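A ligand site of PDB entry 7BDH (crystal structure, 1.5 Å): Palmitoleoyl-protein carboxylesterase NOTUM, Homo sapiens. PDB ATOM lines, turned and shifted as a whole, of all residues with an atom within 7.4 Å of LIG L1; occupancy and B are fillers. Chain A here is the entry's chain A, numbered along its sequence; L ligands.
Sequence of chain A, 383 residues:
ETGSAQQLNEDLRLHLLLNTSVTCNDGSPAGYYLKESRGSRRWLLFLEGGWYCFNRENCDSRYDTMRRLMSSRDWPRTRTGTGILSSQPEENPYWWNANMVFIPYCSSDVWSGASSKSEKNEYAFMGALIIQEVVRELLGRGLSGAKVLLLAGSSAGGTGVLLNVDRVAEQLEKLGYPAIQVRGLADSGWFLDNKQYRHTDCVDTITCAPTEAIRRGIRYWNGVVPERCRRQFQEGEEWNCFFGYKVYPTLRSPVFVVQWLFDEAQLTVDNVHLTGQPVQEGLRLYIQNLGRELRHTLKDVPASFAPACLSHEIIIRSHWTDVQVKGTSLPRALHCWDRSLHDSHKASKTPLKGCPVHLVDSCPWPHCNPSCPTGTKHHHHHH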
ATOM      1  N   TYR A  52       7.468   8.870  19.350  1.00  0.00           N
ATOM      2  CA  TYR A  52       8.100   7.551  19.344  1.00  0.00           C
ATOM      3  C   TYR A  52       9.616   7.751  19.470  1.00  0.00           C
ATOM      4  O   TYR A  52      10.122   8.870  19.404  1.00  0.00           O
ATOM      5  CB  TYR A  52       7.755   6.745  18.071  1.00  0.00           C
ATOM      6  CG  TYR A  52       8.146   7.424  16.760  1.00  0.00           C
ATOM      7  CD1 TYR A  52       9.432   7.288  16.237  1.00  0.00           C
ATOM      8  CD2 TYR A  52       7.231   8.202  16.048  1.00  0.00           C
ATOM      9  CE1 TYR A  52       9.803   7.910  15.052  1.00  0.00           C
ATOM     10  CE2 TYR A  52       7.592   8.827  14.854  1.00  0.00           C
ATOM     11  CZ  TYR A  52       8.879   8.671  14.367  1.00  0.00           C
ATOM     12  OH  TYR A  52       9.277   9.271  13.186  1.00  0.00           O
ATOM     13  N   PHE A 191      -1.079  11.089   8.193  1.00  0.00           N
ATOM     14  CA  PHE A 191       0.077  11.897   7.795  1.00  0.00           C
ATOM     15  C   PHE A 191       0.395  11.767   6.307  1.00  0.00           C
ATOM     16  O   PHE A 191       0.056  10.762   5.666  1.00  0.00           O
ATOM     17  CB  PHE A 191       1.321  11.507   8.620  1.00  0.00           C
ATOM     18  CG  PHE A 191       1.213  11.811  10.100  1.00  0.00           C
ATOM     19  CD1 PHE A 191       0.959  10.795  11.022  1.00  0.00           C
ATOM     20  CD2 PHE A 191       1.405  13.094  10.566  1.00  0.00           C
ATOM     21  CE1 PHE A 191       0.855  11.071  12.382  1.00  0.00           C
ATOM     22  CE2 PHE A 191       1.310  13.373  11.941  1.00  0.00           C
ATOM     23  CZ  PHE A 191       1.028  12.355  12.837  1.00  0.00           C
ATOM     24  N   LEU A 192       1.054  12.779   5.757  1.00  0.00           N
ATOM     25  CA  LEU A 192       1.500  12.775   4.363  1.00  0.00           C
ATOM     26  C   LEU A 192       3.016  12.712   4.307  1.00  0.00           C
ATOM     27  O   LEU A 192       3.695  13.477   5.021  1.00  0.00           O
ATOM     28  CB  LEU A 192       1.002  14.024   3.625  1.00  0.00           C
ATOM     29  CG  LEU A 192      -0.508  14.235   3.529  1.00  0.00           C
ATOM     30  CD1 LEU A 192      -0.804  15.516   2.790  1.00  0.00           C
ATOM     31  CD2 LEU A 192      -1.207  13.045   2.854  1.00  0.00           C
ATOM     32  N   ASP A 193       3.558  11.808   3.483  1.00  0.00           N
ATOM     33  CA  ASP A 193       5.010  11.760   3.247  1.00  0.00           C
ATOM     34  C   ASP A 193       5.383  12.726   2.114  1.00  0.00           C
ATOM     35  O   ASP A 193       5.878  12.349   1.054  1.00  0.00           O
ATOM     36  CB  ASP A 193       5.481  10.327   2.984  1.00  0.00           C
ATOM     37  CG  ASP A 193       4.654   9.579   1.928  1.00  0.00           C
ATOM     38  OD1 ASP A 193       3.536   9.998   1.585  1.00  0.00           O
ATOM     39  OD2 ASP A 193       5.148   8.503   1.456  1.00  0.00           O
ATOM     40  N   ASN A 194       5.114  14.021   2.372  1.00  0.00           N
ATOM     41  CA  ASN A 194       5.242  15.075   1.367  1.00  0.00           C
ATOM     42  C   ASN A 194       6.622  15.746   1.410  1.00  0.00           C
ATOM     43  O   ASN A 194       7.444  15.498   2.288  1.00  0.00           O
ATOM     44  CB  ASN A 194       4.132  16.125   1.538  1.00  0.00           C
ATOM     45  CG  ASN A 194       4.244  16.891   2.835  1.00  0.00           C
ATOM     46  OD1 ASN A 194       4.920  16.477   3.773  1.00  0.00           O
ATOM     47  ND2 ASN A 194       3.570  18.045   2.902  1.00  0.00           N
ATOM     48  N   LYS A 195       6.845  16.616   0.430  1.00  0.00           N
ATOM     49  CA  LYS A 195       8.066  17.404   0.370  1.00  0.00           C
ATOM     50  C   LYS A 195       8.060  18.465   1.475  1.00  0.00           C
ATOM     51  O   LYS A 195       7.061  19.150   1.666  1.00  0.00           O
ATOM     52  CB  LYS A 195       8.200  18.054  -0.999  1.00  0.00           C
ATOM     53  CG  LYS A 195       9.302  19.084  -1.122  1.00  0.00           C
ATOM     54  CD  LYS A 195       8.886  20.174  -2.097  1.00  0.00           C
ATOM     55  CE  LYS A 195       8.361  19.585  -3.405  1.00  0.00           C
ATOM     56  NZ  LYS A 195       7.475  20.548  -4.131  1.00  0.00           N
ATOM     57  N   GLN A 196       9.154  18.564   2.207  1.00  0.00           N
ATOM     58  CA  GLN A 196       9.255  19.529   3.293  1.00  0.00           C
ATOM     59  C   GLN A 196       9.449  20.948   2.743  1.00  0.00           C
ATOM     60  O   GLN A 196       9.928  21.155   1.629  1.00  0.00           O
ATOM     61  CB  GLN A 196      10.407  19.154   4.212  1.00  0.00           C
ATOM     62  CG  GLN A 196      10.257  17.768   4.825  1.00  0.00           C
ATOM     63  CD  GLN A 196      11.533  17.294   5.448  1.00  0.00           C
ATOM     64  OE1 GLN A 196      12.471  16.894   4.751  1.00  0.00           O
ATOM     65  NE2 GLN A 196      11.606  17.356   6.779  1.00  0.00           N
ATOM     66  N   PRO A 210      12.904  12.215   8.337  1.00  0.00           N
ATOM     67  CA  PRO A 210      11.901  11.912   7.328  1.00  0.00           C
ATOM     68  C   PRO A 210      11.344  10.496   7.512  1.00  0.00           C
ATOM     69  O   PRO A 210      11.226  10.007   8.631  1.00  0.00           O
ATOM     70  CB  PRO A 210      12.491  12.092   5.930  1.00  0.00           C
ATOM     71  N   THR A 211      11.005   9.834   6.395  1.00  0.00           N
ATOM     72  CA  THR A 211      10.531   8.457   6.426  1.00  0.00           C
ATOM     73  C   THR A 211      11.617   7.480   6.880  1.00  0.00           C
ATOM     74  O   THR A 211      11.300   6.311   7.145  1.00  0.00           O
ATOM     75  CB  THR A 211      10.032   8.020   5.048  1.00  0.00           C
ATOM     76  OG1 THR A 211      11.035   8.349   4.078  1.00  0.00           O
ATOM     77  CG2 THR A 211       8.728   8.707   4.689  1.00  0.00           C
ATOM     78  N   GLU A 212      12.878   7.923   6.924  1.00  0.00           N
ATOM     79  CA  GLU A 212      13.946   7.054   7.423  1.00  0.00           C
ATOM     80  C   GLU A 212      13.716   6.676   8.875  1.00  0.00           C
ATOM     81  O   GLU A 212      14.078   5.566   9.285  1.00  0.00           O
ATOM     82  CB  GLU A 212      15.301   7.752   7.277  1.00  0.00           C
ATOM     83  CG  GLU A 212      15.981   7.432   5.971  1.00  0.00           C
ATOM     84  CD  GLU A 212      16.155   5.941   5.767  1.00  0.00           C
ATOM     85  OE1 GLU A 212      16.586   5.253   6.723  1.00  0.00           O
ATOM     86  OE2 GLU A 212      15.835   5.455   4.657  1.00  0.00           O
ATOM     87  N   ILE A 214      10.922   6.048  10.495  1.00  0.00           N
ATOM     88  CA  ILE A 214      10.002   4.931  10.566  1.00  0.00           C
ATOM     89  C   ILE A 214      10.651   3.641  10.070  1.00  0.00           C
ATOM     90  O   ILE A 214      10.485   2.582  10.669  1.00  0.00           O
ATOM     91  CB  ILE A 214       8.712   5.250   9.779  1.00  0.00           C
ATOM     92  CG1 ILE A 214       8.015   6.499  10.341  1.00  0.00           C
ATOM     93  CG2 ILE A 214       7.772   4.062   9.777  1.00  0.00           C
ATOM     94  CD1 ILE A 214       7.514   6.332  11.751  1.00  0.00           C
ATOM     95  N   TRP A 239       7.344   0.541   5.853  1.00  0.00           N
ATOM     96  CA  TRP A 239       7.126   1.903   6.367  1.00  0.00           C
ATOM     97  C   TRP A 239       5.951   2.588   5.676  1.00  0.00           C
ATOM     98  O   TRP A 239       5.310   3.478   6.258  1.00  0.00           O
ATOM     99  CB  TRP A 239       8.404   2.754   6.207  1.00  0.00           C
ATOM    100  CG  TRP A 239       8.798   2.969   4.774  1.00  0.00           C
ATOM    101  CD1 TRP A 239       9.688   2.227   4.047  1.00  0.00           C
ATOM    102  CD2 TRP A 239       8.305   3.990   3.897  1.00  0.00           C
ATOM    103  NE1 TRP A 239       9.790   2.733   2.768  1.00  0.00           N
ATOM    104  CE2 TRP A 239       8.947   3.802   2.648  1.00  0.00           C
ATOM    105  CE3 TRP A 239       7.389   5.045   4.030  1.00  0.00           C
ATOM    106  CZ2 TRP A 239       8.691   4.638   1.542  1.00  0.00           C
ATOM    107  CZ3 TRP A 239       7.148   5.864   2.935  1.00  0.00           C
ATOM    108  CH2 TRP A 239       7.783   5.653   1.706  1.00  0.00           C
ATOM    109  N   PHE A 243       1.369   5.249   6.724  1.00  0.00           N
ATOM    110  CA  PHE A 243       0.762   6.439   6.150  1.00  0.00           C
ATOM    111  C   PHE A 243      -0.674   6.137   5.758  1.00  0.00           C
ATOM    112  O   PHE A 243      -0.923   5.273   4.907  1.00  0.00           O
ATOM    113  CB  PHE A 243       1.605   6.960   4.983  1.00  0.00           C
ATOM    114  CG  PHE A 243       2.899   7.555   5.444  1.00  0.00           C
ATOM    115  CD1 PHE A 243       4.005   6.749   5.669  1.00  0.00           C
ATOM    116  CD2 PHE A 243       2.966   8.890   5.784  1.00  0.00           C
ATOM    117  CE1 PHE A 243       5.185   7.290   6.164  1.00  0.00           C
ATOM    118  CE2 PHE A 243       4.138   9.451   6.285  1.00  0.00           C
ATOM    119  CZ  PHE A 243       5.260   8.647   6.470  1.00  0.00           C
ATOM    120  N   ALA A 265       1.445  18.789  13.932  1.00  0.00           N
ATOM    121  CA  ALA A 265       2.557  17.844  13.896  1.00  0.00           C
ATOM    122  C   ALA A 265       3.066  17.650  12.471  1.00  0.00           C
ATOM    123  O   ALA A 265       4.288  17.592  12.245  1.00  0.00           O
ATOM    124  CB  ALA A 265       2.148  16.505  14.522  1.00  0.00           C
ATOM    125  N   GLN A 266       2.153  17.547  11.508  1.00  0.00           N
ATOM    126  CA  GLN A 266       2.534  17.493  10.091  1.00  0.00           C
ATOM    127  C   GLN A 266       3.373  18.701   9.707  1.00  0.00           C
ATOM    128  O   GLN A 266       4.418  18.581   9.057  1.00  0.00           O
ATOM    129  CB  GLN A 266       1.274  17.409   9.221  1.00  0.00           C
ATOM    130  CG  GLN A 266       1.511  17.513   7.725  1.00  0.00           C
ATOM    131  CD  GLN A 266       1.899  16.197   7.106  1.00  0.00           C
ATOM    132  OE1 GLN A 266       1.293  15.158   7.406  1.00  0.00           O
ATOM    133  NE2 GLN A 266       2.910  16.216   6.235  1.00  0.00           N
ATOM    134  N   LEU A 267       2.935  19.901  10.106  1.00  0.00           N
ATOM    135  CA  LEU A 267       3.664  21.115   9.742  1.00  0.00           C
ATOM    136  C   LEU A 267       5.026  21.182  10.434  1.00  0.00           C
ATOM    137  O   LEU A 267       5.987  21.683   9.841  1.00  0.00           O
ATOM    138  CB  LEU A 267       2.814  22.355  10.046  1.00  0.00           C
ATOM    139  CG  LEU A 267       1.722  22.623   9.009  1.00  0.00           C
ATOM    140  CD1 LEU A 267       0.757  23.690   9.472  1.00  0.00           C
ATOM    141  CD2 LEU A 267       2.317  23.030   7.681  1.00  0.00           C
ATOM    142  N   THR A 268       5.130  20.677  11.670  1.00  0.00           N
ATOM    143  CA  THR A 268       6.415  20.655  12.360  1.00  0.00           C
ATOM    144  C   THR A 268       7.425  19.764  11.630  1.00  0.00           C
ATOM    145  O   THR A 268       8.577  20.167  11.409  1.00  0.00           O
ATOM    146  CB  THR A 268       6.235  20.187  13.805  1.00  0.00           C
ATOM    147  OG1 THR A 268       5.482  21.170  14.527  1.00  0.00           O
ATOM    148  CG2 THR A 268       7.594  20.001  14.486  1.00  0.00           C
ATOM    149  N   VAL A 269       6.997  18.568  11.222  1.00  0.00           N
ATOM    150  CA  VAL A 269       7.907  17.712  10.456  1.00  0.00           C
ATOM    151  C   VAL A 269       8.244  18.344   9.109  1.00  0.00           C
ATOM    152  O   VAL A 269       9.339  18.149   8.575  1.00  0.00           O
ATOM    153  CB  VAL A 269       7.326  16.291  10.287  1.00  0.00           C
ATOM    154  CG1 VAL A 269       8.273  15.399   9.485  1.00  0.00           C
ATOM    155  CG2 VAL A 269       7.024  15.648  11.632  1.00  0.00           C
ATOM    156  N   ASP A 270       7.325  19.136   8.546  1.00  0.00           N
ATOM    157  CA  ASP A 270       7.564  19.839   7.292  1.00  0.00           C
ATOM    158  C   ASP A 270       8.456  21.073   7.465  1.00  0.00           C
ATOM    159  O   ASP A 270       8.764  21.746   6.470  1.00  0.00           O
ATOM    160  CB  ASP A 270       6.224  20.255   6.653  1.00  0.00           C
ATOM    161  CG  ASP A 270       5.538  19.104   5.944  1.00  0.00           C
ATOM    162  OD1 ASP A 270       6.262  18.267   5.330  1.00  0.00           O
ATOM    163  OD2 ASP A 270       4.288  19.051   5.939  1.00  0.00           O
ATOM    164  N   ASN A 271       8.883  21.362   8.706  1.00  0.00           N
ATOM    165  CA  ASN A 271       9.762  22.498   9.036  1.00  0.00           C
ATOM    166  C   ASN A 271       9.069  23.834   8.754  1.00  0.00           C
ATOM    167  O   ASN A 271       9.697  24.780   8.272  1.00  0.00           O
ATOM    168  CB  ASN A 271      11.111  22.414   8.321  1.00  0.00           C
ATOM    169  CG  ASN A 271      11.982  21.280   8.854  1.00  0.00           C
ATOM    170  OD1 ASN A 271      12.053  21.061  10.067  1.00  0.00           O
ATOM    171  ND2 ASN A 271      12.617  20.555   7.947  1.00  0.00           N
ATOM    172  N   TYR A 286       2.778  26.794  -0.351  1.00  0.00           N
ATOM    173  CA  TYR A 286       3.047  25.524   0.334  1.00  0.00           C
ATOM    174  C   TYR A 286       1.879  25.111   1.239  1.00  0.00           C
ATOM    175  O   TYR A 286       1.440  23.948   1.215  1.00  0.00           O
ATOM    176  CB  TYR A 286       4.357  25.634   1.154  1.00  0.00           C
ATOM    177  CG  TYR A 286       4.773  24.324   1.782  1.00  0.00           C
ATOM    178  CD1 TYR A 286       5.651  23.456   1.119  1.00  0.00           C
ATOM    179  CD2 TYR A 286       4.265  23.922   3.008  1.00  0.00           C
ATOM    180  CE1 TYR A 286       6.018  22.231   1.681  1.00  0.00           C
ATOM    181  CE2 TYR A 286       4.619  22.700   3.576  1.00  0.00           C
ATOM    182  CZ  TYR A 286       5.489  21.860   2.912  1.00  0.00           C
ATOM    183  OH  TYR A 286       5.830  20.649   3.477  1.00  0.00           O
HETATM  184  C1  LIG L   1       7.056  12.734   6.065  1.00  0.00           C
HETATM  185  C2  LIG L   1       9.690  12.716   2.303  1.00  0.00           C
HETATM  186  C3  LIG L   1       9.010  12.670   3.672  1.00  0.00           C
HETATM  187  C4  LIG L   1       7.358  13.845   5.278  1.00  0.00           C
HETATM  188  C5  LIG L   1       6.837  15.092   5.636  1.00  0.00           C
HETATM  189  C6  LIG L   1       6.056  15.232   6.780  1.00  0.00           C
HETATM  190  C7  LIG L   1       5.779  14.099   7.586  1.00  0.00           C
HETATM  191  C8  LIG L   1       6.261  12.871   7.236  1.00  0.00           C
HETATM  192  N1  LIG L   1       8.115  13.752   4.043  1.00  0.00           N
HETATM  193  N2  LIG L   1       5.937  11.868   8.098  1.00  0.00           N
HETATM  194  N3  LIG L   1       5.020  14.171   8.720  1.00  0.00           N
HETATM  195  O1  LIG L   1       9.222  11.763   4.408  1.00  0.00           O
HETATM  196  S1  LIG L   1       4.988  12.589   9.303  1.00  0.00           S
HETATM  197  C1  LG2 L   2       4.551  10.847  12.587  1.00  0.00           C
HETATM  198  C2  LG2 L   2       6.004  14.013  15.611  1.00  0.00           C
HETATM  199  C3  LG2 L   2       5.815  12.829  14.666  1.00  0.00           C
HETATM  200  C4  LG2 L   2       4.288  10.847  13.964  1.00  0.00           C
HETATM  201  C5  LG2 L   2       3.680   9.726  14.544  1.00  0.00           C
HETATM  202  C6  LG2 L   2       3.350   8.620  13.756  1.00  0.00           C
HETATM  203  C7  LG2 L   2       3.624   8.623  12.366  1.00  0.00           C
HETATM  204  C8  LG2 L   2       4.209   9.714  11.791  1.00  0.00           C
HETATM  205  N1  LG2 L   2       4.617  12.007  14.787  1.00  0.00           N
HETATM  206  N2  LG2 L   2       4.437   9.610  10.446  1.00  0.00           N
HETATM  207  N3  LG2 L   2       3.322   7.581  11.539  1.00  0.00           N
HETATM  208  O1  LG2 L   2       6.658  12.616  13.853  1.00  0.00           O
HETATM  209  S1  LG2 L   2       3.836   8.094  10.018  1.00  0.00           S
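The backbone carbonyl oxygen of Asn 194 sits at hydrogen-bond distance from a nitrogen (N1) of LIG L1, at 2.6 Å. N of Thr 211 lies close to O1 of LIG L1, at 3.3 Å.
Merely in contact with LIG L1: Asp 270 (3.2 Å), Gln 266 (3.3 Å), Leu 192 (3.4 Å), Val 269 (3.4 Å), Asp 193 (3.5 Å), Phe 243 (3.5 Å), Pro 210 (3.6 Å) and Phe 191 (3.8 Å). The nearest printed residue that does not touch LIG L1 is Gln 196 (4.4 Å).
The side-chain amide oxygen (OD1) of Asn 194 lies close to the side-chain carboxylate (OD1) of Asp 270 (2.7 Å). OD1 of Asn 194 is in hydrogen-bond range of NE2 of Gln 266 (3.2 Å). The backbone carbonyl oxygen (O) of Leu 192 sits close to the side-chain amide oxygen (OD1) of Asn 194 (3.5 Å). The side-chain hydroxyl (OH) of Tyr 286 sits at hydrogen-bond distance from the side-chain amide nitrogen (ND2) of Asn 194 (3.5 Å). The side-chain amide nitrogen (NE2) of Gln 266 sits at hydrogen-bond distance from the side-chain carboxylate (OD2) of Asp 270, 3.2 Å away. The side-chain carboxylate (OD1) of Asp 270 sits close to the side-chain hydroxyl (OH) of Tyr 286 (3.0 Å). The side-chain amide oxygen of Gln 266 is in hydrogen-bond range of the backbone NH of Leu 192 (2.9 Å). The side-chain amide nitrogen (NE2) of Gln 196 lies within hydrogen-bond range of the backbone carbonyl oxygen (O) of Val 269 (3.0 Å).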
